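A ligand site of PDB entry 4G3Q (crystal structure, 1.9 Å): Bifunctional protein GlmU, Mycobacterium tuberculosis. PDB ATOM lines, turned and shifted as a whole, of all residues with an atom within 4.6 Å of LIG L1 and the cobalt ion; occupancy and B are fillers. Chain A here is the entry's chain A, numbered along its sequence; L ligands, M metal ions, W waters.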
ATOM      1  N   LEU A  18      11.192 -21.413  -6.344  1.00  0.00           N
ATOM      2  CA  LEU A  18      10.198 -22.218  -5.623  1.00  0.00           C
ATOM      3  C   LEU A  18      10.041 -21.601  -4.282  1.00  0.00           C
ATOM      4  O   LEU A  18      10.995 -21.564  -3.445  1.00  0.00           O
ATOM      5  CB  LEU A  18      10.710 -23.672  -5.473  1.00  0.00           C
ATOM      6  CG  LEU A  18      11.148 -24.346  -6.808  1.00  0.00           C
ATOM      7  CD1 LEU A  18      11.507 -25.820  -6.589  1.00  0.00           C
ATOM      8  CD2 LEU A  18      10.018 -24.242  -7.906  1.00  0.00           C
ATOM      9  N   ALA A  19       8.865 -21.029  -4.043  1.00  0.00           N
ATOM     10  CA  ALA A  19       8.653 -20.346  -2.802  1.00  0.00           C
ATOM     11  C   ALA A  19       7.259 -20.713  -2.264  1.00  0.00           C
ATOM     12  O   ALA A  19       6.629 -19.900  -1.563  1.00  0.00           O
ATOM     13  CB  ALA A  19       8.736 -18.834  -3.028  1.00  0.00           C
ATOM     14  N   ALA A  20       6.780 -21.936  -2.547  1.00  0.00           N
ATOM     15  CA  ALA A  20       5.404 -22.333  -2.132  1.00  0.00           C
ATOM     16  C   ALA A  20       5.316 -23.431  -1.048  1.00  0.00           C
ATOM     17  O   ALA A  20       4.205 -23.918  -0.681  1.00  0.00           O
ATOM     18  CB  ALA A  20       4.596 -22.801  -3.375  1.00  0.00           C
ATOM     19  N   GLY A  21       6.453 -23.760  -0.451  1.00  0.00           N
ATOM     20  CA  GLY A  21       6.446 -24.668   0.692  1.00  0.00           C
ATOM     21  C   GLY A  21       5.870 -23.989   1.935  1.00  0.00           C
ATOM     22  O   GLY A  21       5.817 -22.754   1.996  1.00  0.00           O
ATOM     23  N   ARG A  25       9.361 -25.454   9.614  1.00  0.00           N
ATOM     24  CA  ARG A  25      10.518 -25.406  10.484  1.00  0.00           C
ATOM     25  C   ARG A  25      10.941 -24.011  10.988  1.00  0.00           C
ATOM     26  O   ARG A  25      11.680 -23.906  11.977  1.00  0.00           O
ATOM     27  CB  ARG A  25      11.679 -26.192   9.899  1.00  0.00           C
ATOM     28  CG  ARG A  25      11.456 -27.736   9.954  1.00  0.00           C
ATOM     29  CD  ARG A  25      12.570 -28.435   9.061  1.00  0.00           C
ATOM     30  NE  ARG A  25      12.339 -28.140   7.629  1.00  0.00           N
ATOM     31  CZ  ARG A  25      13.100 -28.613   6.633  1.00  0.00           C
ATOM     32  NH1 ARG A  25      14.214 -29.307   6.933  1.00  0.00           N
ATOM     33  NH2 ARG A  25      12.802 -28.375   5.341  1.00  0.00           N
ATOM     34  N   LYS A  32       7.966 -17.914   5.425  1.00  0.00           N
ATOM     35  CA  LYS A  32       9.434 -18.150   5.471  1.00  0.00           C
ATOM     36  C   LYS A  32      10.214 -17.200   4.563  1.00  0.00           C
ATOM     37  O   LYS A  32      11.229 -16.649   4.978  1.00  0.00           O
ATOM     38  CB  LYS A  32       9.805 -19.555   5.075  1.00  0.00           C
ATOM     39  CG  LYS A  32      11.352 -19.757   4.783  1.00  0.00           C
ATOM     40  CD  LYS A  32      11.941 -21.193   4.983  1.00  0.00           C
ATOM     41  CE  LYS A  32      11.789 -22.090   3.789  1.00  0.00           C
ATOM     42  NZ  LYS A  32      12.575 -23.357   3.946  1.00  0.00           N
ATOM     43  N   VAL A  61       6.920 -19.410  -7.915  1.00  0.00           N
ATOM     44  CA  VAL A  61       5.863 -20.326  -7.498  1.00  0.00           C
ATOM     45  C   VAL A  61       5.501 -20.037  -6.078  1.00  0.00           C
ATOM     46  O   VAL A  61       6.361 -20.111  -5.170  1.00  0.00           O
ATOM     47  CB  VAL A  61       6.354 -21.812  -7.665  1.00  0.00           C
ATOM     48  CG1 VAL A  61       5.250 -22.800  -7.231  1.00  0.00           C
ATOM     49  CG2 VAL A  61       6.816 -22.059  -9.133  1.00  0.00           C
ATOM     50  N   GLN A  89       0.856 -22.948  -6.617  1.00  0.00           N
ATOM     51  CA  GLN A  89       0.871 -24.346  -6.306  1.00  0.00           C
ATOM     52  C   GLN A  89      -0.091 -24.486  -5.151  1.00  0.00           C
ATOM     53  O   GLN A  89       0.210 -24.036  -4.044  1.00  0.00           O
ATOM     54  CB  GLN A  89       2.291 -24.819  -5.906  1.00  0.00           C
ATOM     55  CG  GLN A  89       2.328 -26.328  -5.601  1.00  0.00           C
ATOM     56  CD  GLN A  89       3.605 -26.760  -4.886  1.00  0.00           C
ATOM     57  OE1 GLN A  89       4.214 -25.956  -4.179  1.00  0.00           O
ATOM     58  NE2 GLN A  89       3.960 -28.061  -5.001  1.00  0.00           N
ATOM     59  N   PRO A  92       1.322 -28.074  -1.090  1.00  0.00           N
ATOM     60  CA  PRO A  92       2.771 -28.264  -1.162  1.00  0.00           C
ATOM     61  C   PRO A  92       3.141 -29.742  -1.381  1.00  0.00           C
ATOM     62  O   PRO A  92       3.638 -30.409  -0.491  1.00  0.00           O
ATOM     63  CB  PRO A  92       3.238 -27.733   0.199  1.00  0.00           C
ATOM     64  CG  PRO A  92       2.043 -28.078   1.149  1.00  0.00           C
ATOM     65  CD  PRO A  92       0.866 -27.738   0.279  1.00  0.00           C
ATOM     66  N   LEU A  93       2.967 -30.254  -2.601  1.00  0.00           N
ATOM     67  CA  LEU A  93       3.128 -31.680  -2.809  1.00  0.00           C
ATOM     68  C   LEU A  93       4.592 -32.047  -2.986  1.00  0.00           C
ATOM     69  O   LEU A  93       4.906 -33.243  -3.159  1.00  0.00           O
ATOM     70  CB  LEU A  93       2.359 -32.140  -4.074  1.00  0.00           C
ATOM     71  CG  LEU A  93       0.815 -31.971  -4.093  1.00  0.00           C
ATOM     72  CD1 LEU A  93       0.214 -32.808  -5.236  1.00  0.00           C
ATOM     73  CD2 LEU A  93       0.122 -32.334  -2.812  1.00  0.00           C
ATOM     74  N   GLY A  94       5.456 -31.021  -3.031  1.00  0.00           N
ATOM     75  CA  GLY A  94       6.891 -31.288  -3.037  1.00  0.00           C
ATOM     76  C   GLY A  94       7.594 -30.409  -4.090  1.00  0.00           C
ATOM     77  O   GLY A  94       6.965 -29.791  -4.957  1.00  0.00           O
ATOM     78  N   THR A  95       8.924 -30.350  -4.018  1.00  0.00           N
ATOM     79  CA  THR A  95       9.653 -29.491  -4.973  1.00  0.00           C
ATOM     80  C   THR A  95       9.445 -29.861  -6.446  1.00  0.00           C
ATOM     81  O   THR A  95       9.454 -28.983  -7.322  1.00  0.00           O
ATOM     82  CB  THR A  95      11.131 -29.443  -4.658  1.00  0.00           C
ATOM     83  OG1 THR A  95      11.669 -30.796  -4.533  1.00  0.00           O
ATOM     84  CG2 THR A  95      11.326 -28.696  -3.285  1.00  0.00           C
ATOM     85  N   ALA A  98       6.208 -28.456  -7.419  1.00  0.00           N
ATOM     86  CA  ALA A  98       6.286 -26.989  -7.532  1.00  0.00           C
ATOM     87  C   ALA A  98       6.894 -26.603  -8.883  1.00  0.00           C
ATOM     88  O   ALA A  98       6.427 -25.632  -9.497  1.00  0.00           O
ATOM     89  CB  ALA A  98       7.207 -26.473  -6.336  1.00  0.00           C
ATOM     90  N   SER A 118      15.562 -22.161  -5.117  1.00  0.00           N
ATOM     91  CA  SER A 118      14.602 -22.036  -4.019  1.00  0.00           C
ATOM     92  C   SER A 118      14.597 -20.583  -3.535  1.00  0.00           C
ATOM     93  O   SER A 118      15.600 -19.837  -3.662  1.00  0.00           O
ATOM     94  CB  SER A 118      15.054 -22.933  -2.858  1.00  0.00           C
ATOM     95  OG  SER A 118      15.274 -24.258  -3.334  1.00  0.00           O
ATOM     96  N   GLY A 119      13.528 -20.228  -2.880  1.00  0.00           N
ATOM     97  CA  GLY A 119      13.402 -18.934  -2.259  1.00  0.00           C
ATOM     98  C   GLY A 119      14.144 -18.895  -0.951  1.00  0.00           C
ATOM     99  O   GLY A 119      14.253 -17.839  -0.390  1.00  0.00           O
ATOM    100  N   ASP A 120      14.697 -20.028  -0.494  1.00  0.00           N
ATOM    101  CA  ASP A 120      15.390 -19.974   0.777  1.00  0.00           C
ATOM    102  C   ASP A 120      16.935 -20.120   0.673  1.00  0.00           C
ATOM    103  O   ASP A 120      17.562 -20.580   1.620  1.00  0.00           O
ATOM    104  CB  ASP A 120      14.766 -20.981   1.775  1.00  0.00           C
ATOM    105  CG  ASP A 120      14.978 -22.452   1.334  1.00  0.00           C
ATOM    106  OD1 ASP A 120      15.609 -22.656   0.250  1.00  0.00           O
ATOM    107  OD2 ASP A 120      14.534 -23.365   2.062  1.00  0.00           O
ATOM    108  N   THR A 121      17.503 -19.776  -0.508  1.00  0.00           N
ATOM    109  CA  THR A 121      18.979 -19.736  -0.741  1.00  0.00           C
ATOM    110  C   THR A 121      19.398 -18.295  -1.024  1.00  0.00           C
ATOM    111  O   THR A 121      19.611 -17.911  -2.184  1.00  0.00           O
ATOM    112  CB  THR A 121      19.335 -20.737  -1.932  1.00  0.00           C
ATOM    113  OG1 THR A 121      18.796 -22.046  -1.598  1.00  0.00           O
ATOM    114  CG2 THR A 121      20.836 -20.880  -2.118  1.00  0.00           C
ATOM    115  N   GLY A 155      20.416 -32.222   6.683  1.00  0.00           N
ATOM    116  CA  GLY A 155      19.197 -31.637   6.129  1.00  0.00           C
ATOM    117  C   GLY A 155      19.294 -31.397   4.646  1.00  0.00           C
ATOM    118  O   GLY A 155      18.273 -31.172   3.987  1.00  0.00           O
ATOM    119  N   TYR A 156      20.517 -31.458   4.077  1.00  0.00           N
ATOM    120  CA  TYR A 156      20.709 -31.351   2.645  1.00  0.00           C
ATOM    121  C   TYR A 156      20.547 -32.725   1.934  1.00  0.00           C
ATOM    122  O   TYR A 156      20.846 -33.753   2.523  1.00  0.00           O
ATOM    123  CB  TYR A 156      22.152 -30.860   2.316  1.00  0.00           C
ATOM    124  CG  TYR A 156      22.364 -29.391   2.633  1.00  0.00           C
ATOM    125  CD1 TYR A 156      22.166 -28.417   1.632  1.00  0.00           C
ATOM    126  CD2 TYR A 156      22.781 -28.987   3.891  1.00  0.00           C
ATOM    127  CE1 TYR A 156      22.318 -27.044   1.924  1.00  0.00           C
ATOM    128  CE2 TYR A 156      22.952 -27.601   4.179  1.00  0.00           C
ATOM    129  CZ  TYR A 156      22.766 -26.666   3.169  1.00  0.00           C
ATOM    130  OH  TYR A 156      22.905 -25.349   3.459  1.00  0.00           O
ATOM    131  N   GLY A 157      20.185 -32.693   0.661  1.00  0.00           N
ATOM    132  CA  GLY A 157      20.240 -33.871  -0.206  1.00  0.00           C
ATOM    133  C   GLY A 157      21.722 -34.174  -0.440  1.00  0.00           C
ATOM    134  O   GLY A 157      22.568 -33.251  -0.602  1.00  0.00           O
ATOM    135  N   ILE A 170      20.506 -38.080  -6.054  1.00  0.00           N
ATOM    136  CA  ILE A 170      20.538 -37.207  -4.872  1.00  0.00           C
ATOM    137  C   ILE A 170      19.591 -37.923  -3.871  1.00  0.00           C
ATOM    138  O   ILE A 170      18.451 -38.302  -4.270  1.00  0.00           O
ATOM    139  CB  ILE A 170      20.001 -35.810  -5.186  1.00  0.00           C
ATOM    140  CG1 ILE A 170      21.030 -35.110  -6.113  1.00  0.00           C
ATOM    141  CG2 ILE A 170      19.776 -35.036  -3.841  1.00  0.00           C
ATOM    142  CD1 ILE A 170      20.485 -33.851  -6.794  1.00  0.00           C
ATOM    143  N   GLU A 172      17.680 -37.628  -0.170  1.00  0.00           N
ATOM    144  CA  GLU A 172      17.345 -36.654   0.922  1.00  0.00           C
ATOM    145  C   GLU A 172      17.723 -37.091   2.305  1.00  0.00           C
ATOM    146  O   GLU A 172      17.741 -38.286   2.584  1.00  0.00           O
ATOM    147  CB  GLU A 172      15.854 -36.397   0.910  1.00  0.00           C
ATOM    148  CG  GLU A 172      15.455 -35.663  -0.391  1.00  0.00           C
ATOM    149  CD  GLU A 172      16.156 -34.300  -0.523  1.00  0.00           C
ATOM    150  OE1 GLU A 172      15.747 -33.353   0.180  1.00  0.00           O
ATOM    151  OE2 GLU A 172      17.076 -34.165  -1.359  1.00  0.00           O
ATOM    152  N   ASN A 187      23.542 -31.205  -2.313  1.00  0.00           N
ATOM    153  CA  ASN A 187      22.804 -30.571  -3.337  1.00  0.00           C
ATOM    154  C   ASN A 187      22.479 -29.154  -2.915  1.00  0.00           C
ATOM    155  O   ASN A 187      21.819 -28.941  -1.833  1.00  0.00           O
ATOM    156  CB  ASN A 187      21.480 -31.365  -3.527  1.00  0.00           C
ATOM    157  CG  ASN A 187      20.550 -30.726  -4.500  1.00  0.00           C
ATOM    158  OD1 ASN A 187      20.981 -30.103  -5.468  1.00  0.00           O
ATOM    159  ND2 ASN A 187      19.214 -30.905  -4.284  1.00  0.00           N
ATOM    160  N   ALA A 188      22.860 -28.175  -3.749  1.00  0.00           N
ATOM    161  CA  ALA A 188      22.460 -26.789  -3.555  1.00  0.00           C
ATOM    162  C   ALA A 188      20.989 -26.526  -3.760  1.00  0.00           C
ATOM    163  O   ALA A 188      20.452 -25.485  -3.318  1.00  0.00           O
ATOM    164  CB  ALA A 188      23.249 -25.877  -4.551  1.00  0.00           C
ATOM    165  N   GLY A 189      20.352 -27.393  -4.549  1.00  0.00           N
ATOM    166  CA  GLY A 189      18.997 -27.149  -5.018  1.00  0.00           C
ATOM    167  C   GLY A 189      18.943 -26.016  -6.054  1.00  0.00           C
ATOM    168  O   GLY A 189      17.921 -25.323  -6.142  1.00  0.00           O
ATOM    169  N   TYR A 191      19.528 -25.634 -10.160  1.00  0.00           N
ATOM    170  CA  TYR A 191      19.707 -26.526 -11.316  1.00  0.00           C
ATOM    171  C   TYR A 191      19.507 -25.768 -12.593  1.00  0.00           C
ATOM    172  O   TYR A 191      18.735 -24.808 -12.612  1.00  0.00           O
ATOM    173  CB  TYR A 191      18.592 -27.577 -11.354  1.00  0.00           C
ATOM    174  CG  TYR A 191      18.261 -28.267 -10.032  1.00  0.00           C
ATOM    175  CD1 TYR A 191      17.509 -27.611  -9.046  1.00  0.00           C
ATOM    176  CD2 TYR A 191      18.690 -29.560  -9.797  1.00  0.00           C
ATOM    177  CE1 TYR A 191      17.161 -28.266  -7.817  1.00  0.00           C
ATOM    178  CE2 TYR A 191      18.367 -30.197  -8.576  1.00  0.00           C
ATOM    179  CZ  TYR A 191      17.601 -29.536  -7.618  1.00  0.00           C
ATOM    180  OH  TYR A 191      17.278 -30.201  -6.465  1.00  0.00           O
ATOM    181  N   TYR A 215       9.684 -35.335  -5.096  1.00  0.00           N
ATOM    182  CA  TYR A 215      10.984 -34.663  -4.937  1.00  0.00           C
ATOM    183  C   TYR A 215      11.608 -34.249  -6.276  1.00  0.00           C
ATOM    184  O   TYR A 215      11.841 -35.108  -7.132  1.00  0.00           O
ATOM    185  CB  TYR A 215      11.978 -35.650  -4.352  1.00  0.00           C
ATOM    186  CG  TYR A 215      11.818 -36.113  -2.944  1.00  0.00           C
ATOM    187  CD1 TYR A 215      11.068 -35.391  -2.014  1.00  0.00           C
ATOM    188  CD2 TYR A 215      12.473 -37.296  -2.523  1.00  0.00           C
ATOM    189  CE1 TYR A 215      11.005 -35.852  -0.626  1.00  0.00           C
ATOM    190  CE2 TYR A 215      12.406 -37.772  -1.211  1.00  0.00           C
ATOM    191  CZ  TYR A 215      11.647 -37.040  -0.261  1.00  0.00           C
ATOM    192  OH  TYR A 215      11.633 -37.484   1.071  1.00  0.00           O
ATOM    193  N   LEU A 216      11.957 -32.966  -6.442  1.00  0.00           N
ATOM    194  CA  LEU A 216      12.664 -32.555  -7.654  1.00  0.00           C
ATOM    195  C   LEU A 216      13.925 -33.365  -7.765  1.00  0.00           C
ATOM    196  O   LEU A 216      14.393 -33.683  -8.877  1.00  0.00           O
ATOM    197  CB  LEU A 216      12.954 -31.046  -7.635  1.00  0.00           C
ATOM    198  CG  LEU A 216      13.704 -30.475  -8.847  1.00  0.00           C
ATOM    199  CD1 LEU A 216      12.882 -30.792 -10.161  1.00  0.00           C
ATOM    200  CD2 LEU A 216      13.844 -28.962  -8.600  1.00  0.00           C
ATOM    201  N   THR A 217      14.480 -33.731  -6.608  1.00  0.00           N
ATOM    202  CA  THR A 217      15.800 -34.336  -6.613  1.00  0.00           C
ATOM    203  C   THR A 217      15.792 -35.684  -7.329  1.00  0.00           C
ATOM    204  O   THR A 217      16.852 -36.126  -7.813  1.00  0.00           O
ATOM    205  CB  THR A 217      16.376 -34.499  -5.209  1.00  0.00           C
ATOM    206  OG1 THR A 217      15.336 -35.040  -4.341  1.00  0.00           O
ATOM    207  CG2 THR A 217      16.755 -33.074  -4.611  1.00  0.00           C
ATOM    208  N   GLY A 243      21.334 -23.144   2.316  1.00  0.00           N
ATOM    209  CA  GLY A 243      19.879 -22.962   2.447  1.00  0.00           C
ATOM    210  C   GLY A 243      19.458 -22.616   3.864  1.00  0.00           C
ATOM    211  O   GLY A 243      20.265 -22.744   4.821  1.00  0.00           O
ATOM    212  N   VAL A 244      18.212 -22.092   3.992  1.00  0.00           N
ATOM    213  CA  VAL A 244      17.680 -21.634   5.280  1.00  0.00           C
ATOM    214  C   VAL A 244      16.377 -22.305   5.473  1.00  0.00           C
ATOM    215  O   VAL A 244      15.385 -21.926   4.812  1.00  0.00           O
ATOM    216  CB  VAL A 244      17.492 -20.044   5.323  1.00  0.00           C
ATOM    217  CG1 VAL A 244      16.788 -19.584   6.590  1.00  0.00           C
ATOM    218  CG2 VAL A 244      18.924 -19.259   5.121  1.00  0.00           C
ATOM    219  N   ASN A 245      16.347 -23.328   6.315  1.00  0.00           N
ATOM    220  CA  ASN A 245      15.071 -23.983   6.685  1.00  0.00           C
ATOM    221  C   ASN A 245      14.576 -23.640   8.074  1.00  0.00           C
ATOM    222  O   ASN A 245      13.438 -23.973   8.451  1.00  0.00           O
ATOM    223  CB  ASN A 245      15.148 -25.524   6.592  1.00  0.00           C
ATOM    224  CG  ASN A 245      15.284 -26.003   5.176  1.00  0.00           C
ATOM    225  OD1 ASN A 245      14.872 -25.291   4.262  1.00  0.00           O
ATOM    226  ND2 ASN A 245      15.944 -27.167   4.975  1.00  0.00           N
HETATM  227  C1  LIG L   1      15.772 -28.955  -0.804  1.00  0.00           C
HETATM  228  C2  LIG L   1      16.286 -30.223  -1.597  1.00  0.00           C
HETATM  229  C3  LIG L   1      17.629 -30.713  -1.021  1.00  0.00           C
HETATM  230  C4  LIG L   1      18.653 -29.550  -1.036  1.00  0.00           C
HETATM  231  C5  LIG L   1      18.077 -28.342  -0.267  1.00  0.00           C
HETATM  232  C6  LIG L   1      19.066 -27.164  -0.507  1.00  0.00           C
HETATM  233  C7  LIG L   1      14.300 -31.462  -2.451  1.00  0.00           C
HETATM  234  C8  LIG L   1      13.440 -32.719  -2.285  1.00  0.00           C
HETATM  235  N1  LIG L   1      15.322 -31.334  -1.568  1.00  0.00           N
HETATM  236  O1  LIG L   1      15.649 -29.413   0.558  1.00  0.00           O
HETATM  237  O2  LIG L   1      18.141 -31.813  -1.854  1.00  0.00           O
HETATM  238  O3  LIG L   1      19.880 -30.023  -0.424  1.00  0.00           O
HETATM  239  O4  LIG L   1      16.787 -27.952  -0.782  1.00  0.00           O
HETATM  240  O5  LIG L   1      18.619 -26.012   0.268  1.00  0.00           O
HETATM  241  O6  LIG L   1      14.091 -30.639  -3.333  1.00  0.00           O
HETATM  242  N2  LIG L   1       8.683 -25.635  -2.072  1.00  0.00           N
HETATM  243  C9  LIG L   1       7.561 -25.454  -2.910  1.00  0.00           C
HETATM  244  N3  LIG L   1       6.551 -26.366  -2.882  1.00  0.00           N
HETATM  245  C10 LIG L   1       6.669 -27.505  -2.170  1.00  0.00           C
HETATM  246  C11 LIG L   1       7.799 -27.751  -1.340  1.00  0.00           C
HETATM  247  C12 LIG L   1       8.845 -26.780  -1.320  1.00  0.00           C
HETATM  248  O7  LIG L   1       7.451 -24.426  -3.641  1.00  0.00           O
HETATM  249  O8  LIG L   1       5.715 -28.328  -2.261  1.00  0.00           O
HETATM  250  C13 LIG L   1       9.740 -24.620  -2.103  1.00  0.00           C
HETATM  251  C14 LIG L   1      10.104 -24.110  -0.637  1.00  0.00           C
HETATM  252  O9  LIG L   1       9.300 -22.947  -0.522  1.00  0.00           O
HETATM  253  C15 LIG L   1      11.585 -23.818  -0.716  1.00  0.00           C
HETATM  254  C16 LIG L   1      12.055 -24.792  -1.808  1.00  0.00           C
HETATM  255  O10 LIG L   1      10.906 -25.284  -2.546  1.00  0.00           O
HETATM  256  O11 LIG L   1      11.886 -22.483  -1.174  1.00  0.00           O
HETATM  257  C17 LIG L   1      12.832 -25.990  -1.268  1.00  0.00           C
HETATM  258  O12 LIG L   1      11.959 -26.674  -0.374  1.00  0.00           O
HETATM  259  P1  LIG L   1      12.436 -26.974   1.121  1.00  0.00           P
HETATM  260  O13 LIG L   1      11.342 -27.635   1.891  1.00  0.00           O
HETATM  261  O14 LIG L   1      13.154 -25.882   1.821  1.00  0.00           O
HETATM  262  O15 LIG L   1      13.495 -28.171   0.806  1.00  0.00           O
HETATM  263  P2  LIG L   1      14.792 -28.635   1.636  1.00  0.00           P
HETATM  264  O16 LIG L   1      15.533 -27.398   2.114  1.00  0.00           O
HETATM  265  O17 LIG L   1      14.378 -29.588   2.687  1.00  0.00           O
HETATM  266  P1  LG2 L   2       7.193 -28.947   6.870  1.00  0.00           P
HETATM  267  O1  LG2 L   2       5.695 -28.825   6.999  1.00  0.00           O
HETATM  268  O2  LG2 L   2       7.858 -29.215   8.183  1.00  0.00           O
HETATM  269  O3  LG2 L   2       7.532 -29.980   5.828  1.00  0.00           O
HETATM  270  O4  LG2 L   2       7.708 -27.478   6.407  1.00  0.00           O
HETATM  271  P2  LG2 L   2       9.144 -27.116   5.724  1.00  0.00           P
HETATM  272  O5  LG2 L   2       8.739 -26.132   4.693  1.00  0.00           O
HETATM  273  O6  LG2 L   2       9.886 -28.298   5.168  1.00  0.00           O
HETATM  274  O7  LG2 L   2      10.036 -26.508   6.825  1.00  0.00           O
HETATM  275 CO    CO M   1      15.116 -25.386   2.128  1.00  0.00          CO
HETATM  276 MG    MG M   2       9.199 -30.049   4.555  1.00  0.00          MG
HETATM  277  O   HOH W   1      10.906 -29.949   3.030  1.00  0.00           O
HETATM  278  O   HOH W   2      15.816 -30.563   4.779  1.00  0.00           O
HETATM  279  O   HOH W   3      20.528 -24.400  -0.757  1.00  0.00           O
HETATM  280  O   HOH W   4      17.202 -25.064   2.528  1.00  0.00           O
HETATM  281  O   HOH W   5      15.558 -28.934  -4.930  1.00  0.00           O
HETATM  282  O   HOH W   6      13.661 -32.066   1.666  1.00  0.00           O
HETATM  283  O   HOH W   7      12.191 -29.952  -0.504  1.00  0.00           O
HETATM  284  O   HOH W   8       9.569 -29.889   0.429  1.00  0.00           O
HETATM  285  O   HOH W   9      15.727 -25.304   0.000  1.00  0.00           O
HETATM  286  O   HOH W  10       8.771 -26.851   2.193  1.00  0.00           O
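NZ of Lys 32 touches the cobalt ion, at 3.7 Å.
Within 4 Å of the cobalt ion: Lys 32, Asp 120 and Asn 245.
Along chain A the residues within 4 Å of the cobalt ion span positions 32 to 245.
The nearest printed residue that does not touch the cobalt ion is Val 244 (4.4 Å).
N of Gly 119 is in hydrogen-bond range of O11 of LIG L1, 3.3 Å away.
An oxygen (O7) of LG2 L2 sits at hydrogen-bond distance from the backbone NH (N) of Arg 25, at 3.1 Å.
The backbone carbonyl oxygen (O) of Asn 187 sits at hydrogen-bond distance from an oxygen (O3) of LIG L1, 2.6 Å away.
The backbone carbonyl oxygen (O) of Leu 18 lies within hydrogen-bond range of an oxygen (O11) of LIG L1 (2.6 Å).
The backbone NH (N) of Leu 93 lies within hydrogen-bond range of an oxygen (O8) of LIG L1, 3.4 Å away.
NE of Arg 25 is in salt-bridge range of O7 of LG2 L2 (2.9 Å).
The backbone NH (N) of Gly 21 is in hydrogen-bond range of an oxygen (O9) of LIG L1.
O6 of LIG L1 lies within hydrogen-bond range of OG1 of Thr 95 (2.7 Å).
O2 of LIG L1 lies within hydrogen-bond range of ND2 of Asn 187, at 2.8 Å.
NZ of Lys 32 lies close to O14 of LIG L1.
O3 of LIG L1 is in hydrogen-bond range of N of Gly 157 (2.9 Å).
O7 of LIG L1 is in hydrogen-bond range of N of Ala 20 (2.8 Å).
The guanidinium group of Arg 25 lies within salt-bridge range of an oxygen (O17) of LIG L1.
An oxygen (O2) of LIG L1 is in hydrogen-bond range of the side-chain carboxylate (OE2) of Glu 172, at 2.6 Å.
The backbone NH (N) of Gly 94 lies within hydrogen-bond range of an oxygen (O8) of LIG L1, 2.8 Å away.
N3 of LIG L1 sits at hydrogen-bond distance from OE1 of Gln 89, at 2.7 Å.
The side-chain amide nitrogen (ND2) of Asn 245 sits close to the guanidinium group (NH1) of Arg 25, 3.4 Å away.
The side-chain amino group (NZ) of Lys 32 lies within hydrogen-bond range of the backbone carbonyl oxygen (O) of Val 244.
O of Val 61 sits at hydrogen-bond distance from N of Ala 20 (3.2 Å).
N of Gly 243 lies within hydrogen-bond range of OH of Tyr 156, at 2.9 Å.
OD2 of Asp 120 lies close to NZ of Lys 32, at 2.7 Å.
The side-chain amide oxygen of Asn 187 sits at hydrogen-bond distance from the backbone NH of Gly 189 (2.9 Å).
The side-chain amide nitrogen (ND2) of Asn 187 is in hydrogen-bond range of the side-chain hydroxyl (OH) of Tyr 191 (3.0 Å).
The side-chain amide nitrogen (NE2) of Gln 89 lies close to the backbone NH (N) of Ala 98, 3.3 Å away.
Water W9 bridges the side-chain carboxylate of Asp 120 and an oxygen (O4) of LIG L1.
Water W4 lies within hydrogen-bond range of an oxygen (O5) of LIG L1 (2.8 Å), the side-chain amide nitrogen (ND2) of Asn 245 (3.5 Å) and the backbone NH (N) of Val 244 (3.5 Å).
Water W1 lies within hydrogen-bond range of O13 of LIG L1 (2.6 Å) and NH2 of Arg 25 (3.4 Å).
Water W3 lies within hydrogen-bond range of O5 of LIG L1 (2.7 Å), O of Ala 188 (2.8 Å), OG1 of Thr 121 (3.0 Å) and N of Gly 243 (3.4 Å).
Water W10 bridges an oxygen (O5) of LG2 L2 (2.6 Å) and an oxygen (O13) of LIG L1 (2.7 Å).
Water W2 lies within hydrogen-bond range of the backbone carbonyl oxygen of Gly 155, an oxygen (O17) of LIG L1, the guanidinium group of Arg 25 and the side-chain amide nitrogen of Asn 245.
The cobalt ion is bound by an oxygen (O14) of LIG L1, an oxygen (O16) of LIG L1, the side-chain carboxylate of Asp 120, water W4, the side-chain amide oxygen of Asn 245 and water W9.
The cobalt ion has six donor atoms within binding distance.
An oxygen (O8) of LIG L1 sits close to the backbone carbonyl oxygen (O) of Pro 92 (3.4 Å).
Ala 19 touches LIG L1.
CB of Ala 98 touches O7 of LIG L1 (3.4 Å).
Ser 118 touches LIG L1.
CA of Tyr 156 touches O3 of LIG L1, 3.4 Å away.
Ala 188 touches LIG L1.
Tyr 215 touches LIG L1 (CD1 to C8, 3.6 Å).
CG2 of Thr 217 touches O2 of LIG L1, at 3.3 Å.
Gly 243 touches LIG L1.
Of the 32 residues printed, 24 come within 4 Å of LIG L1.
The nearest printed residue that does not touch LIG L1 is Ile 170 (4.1 Å).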
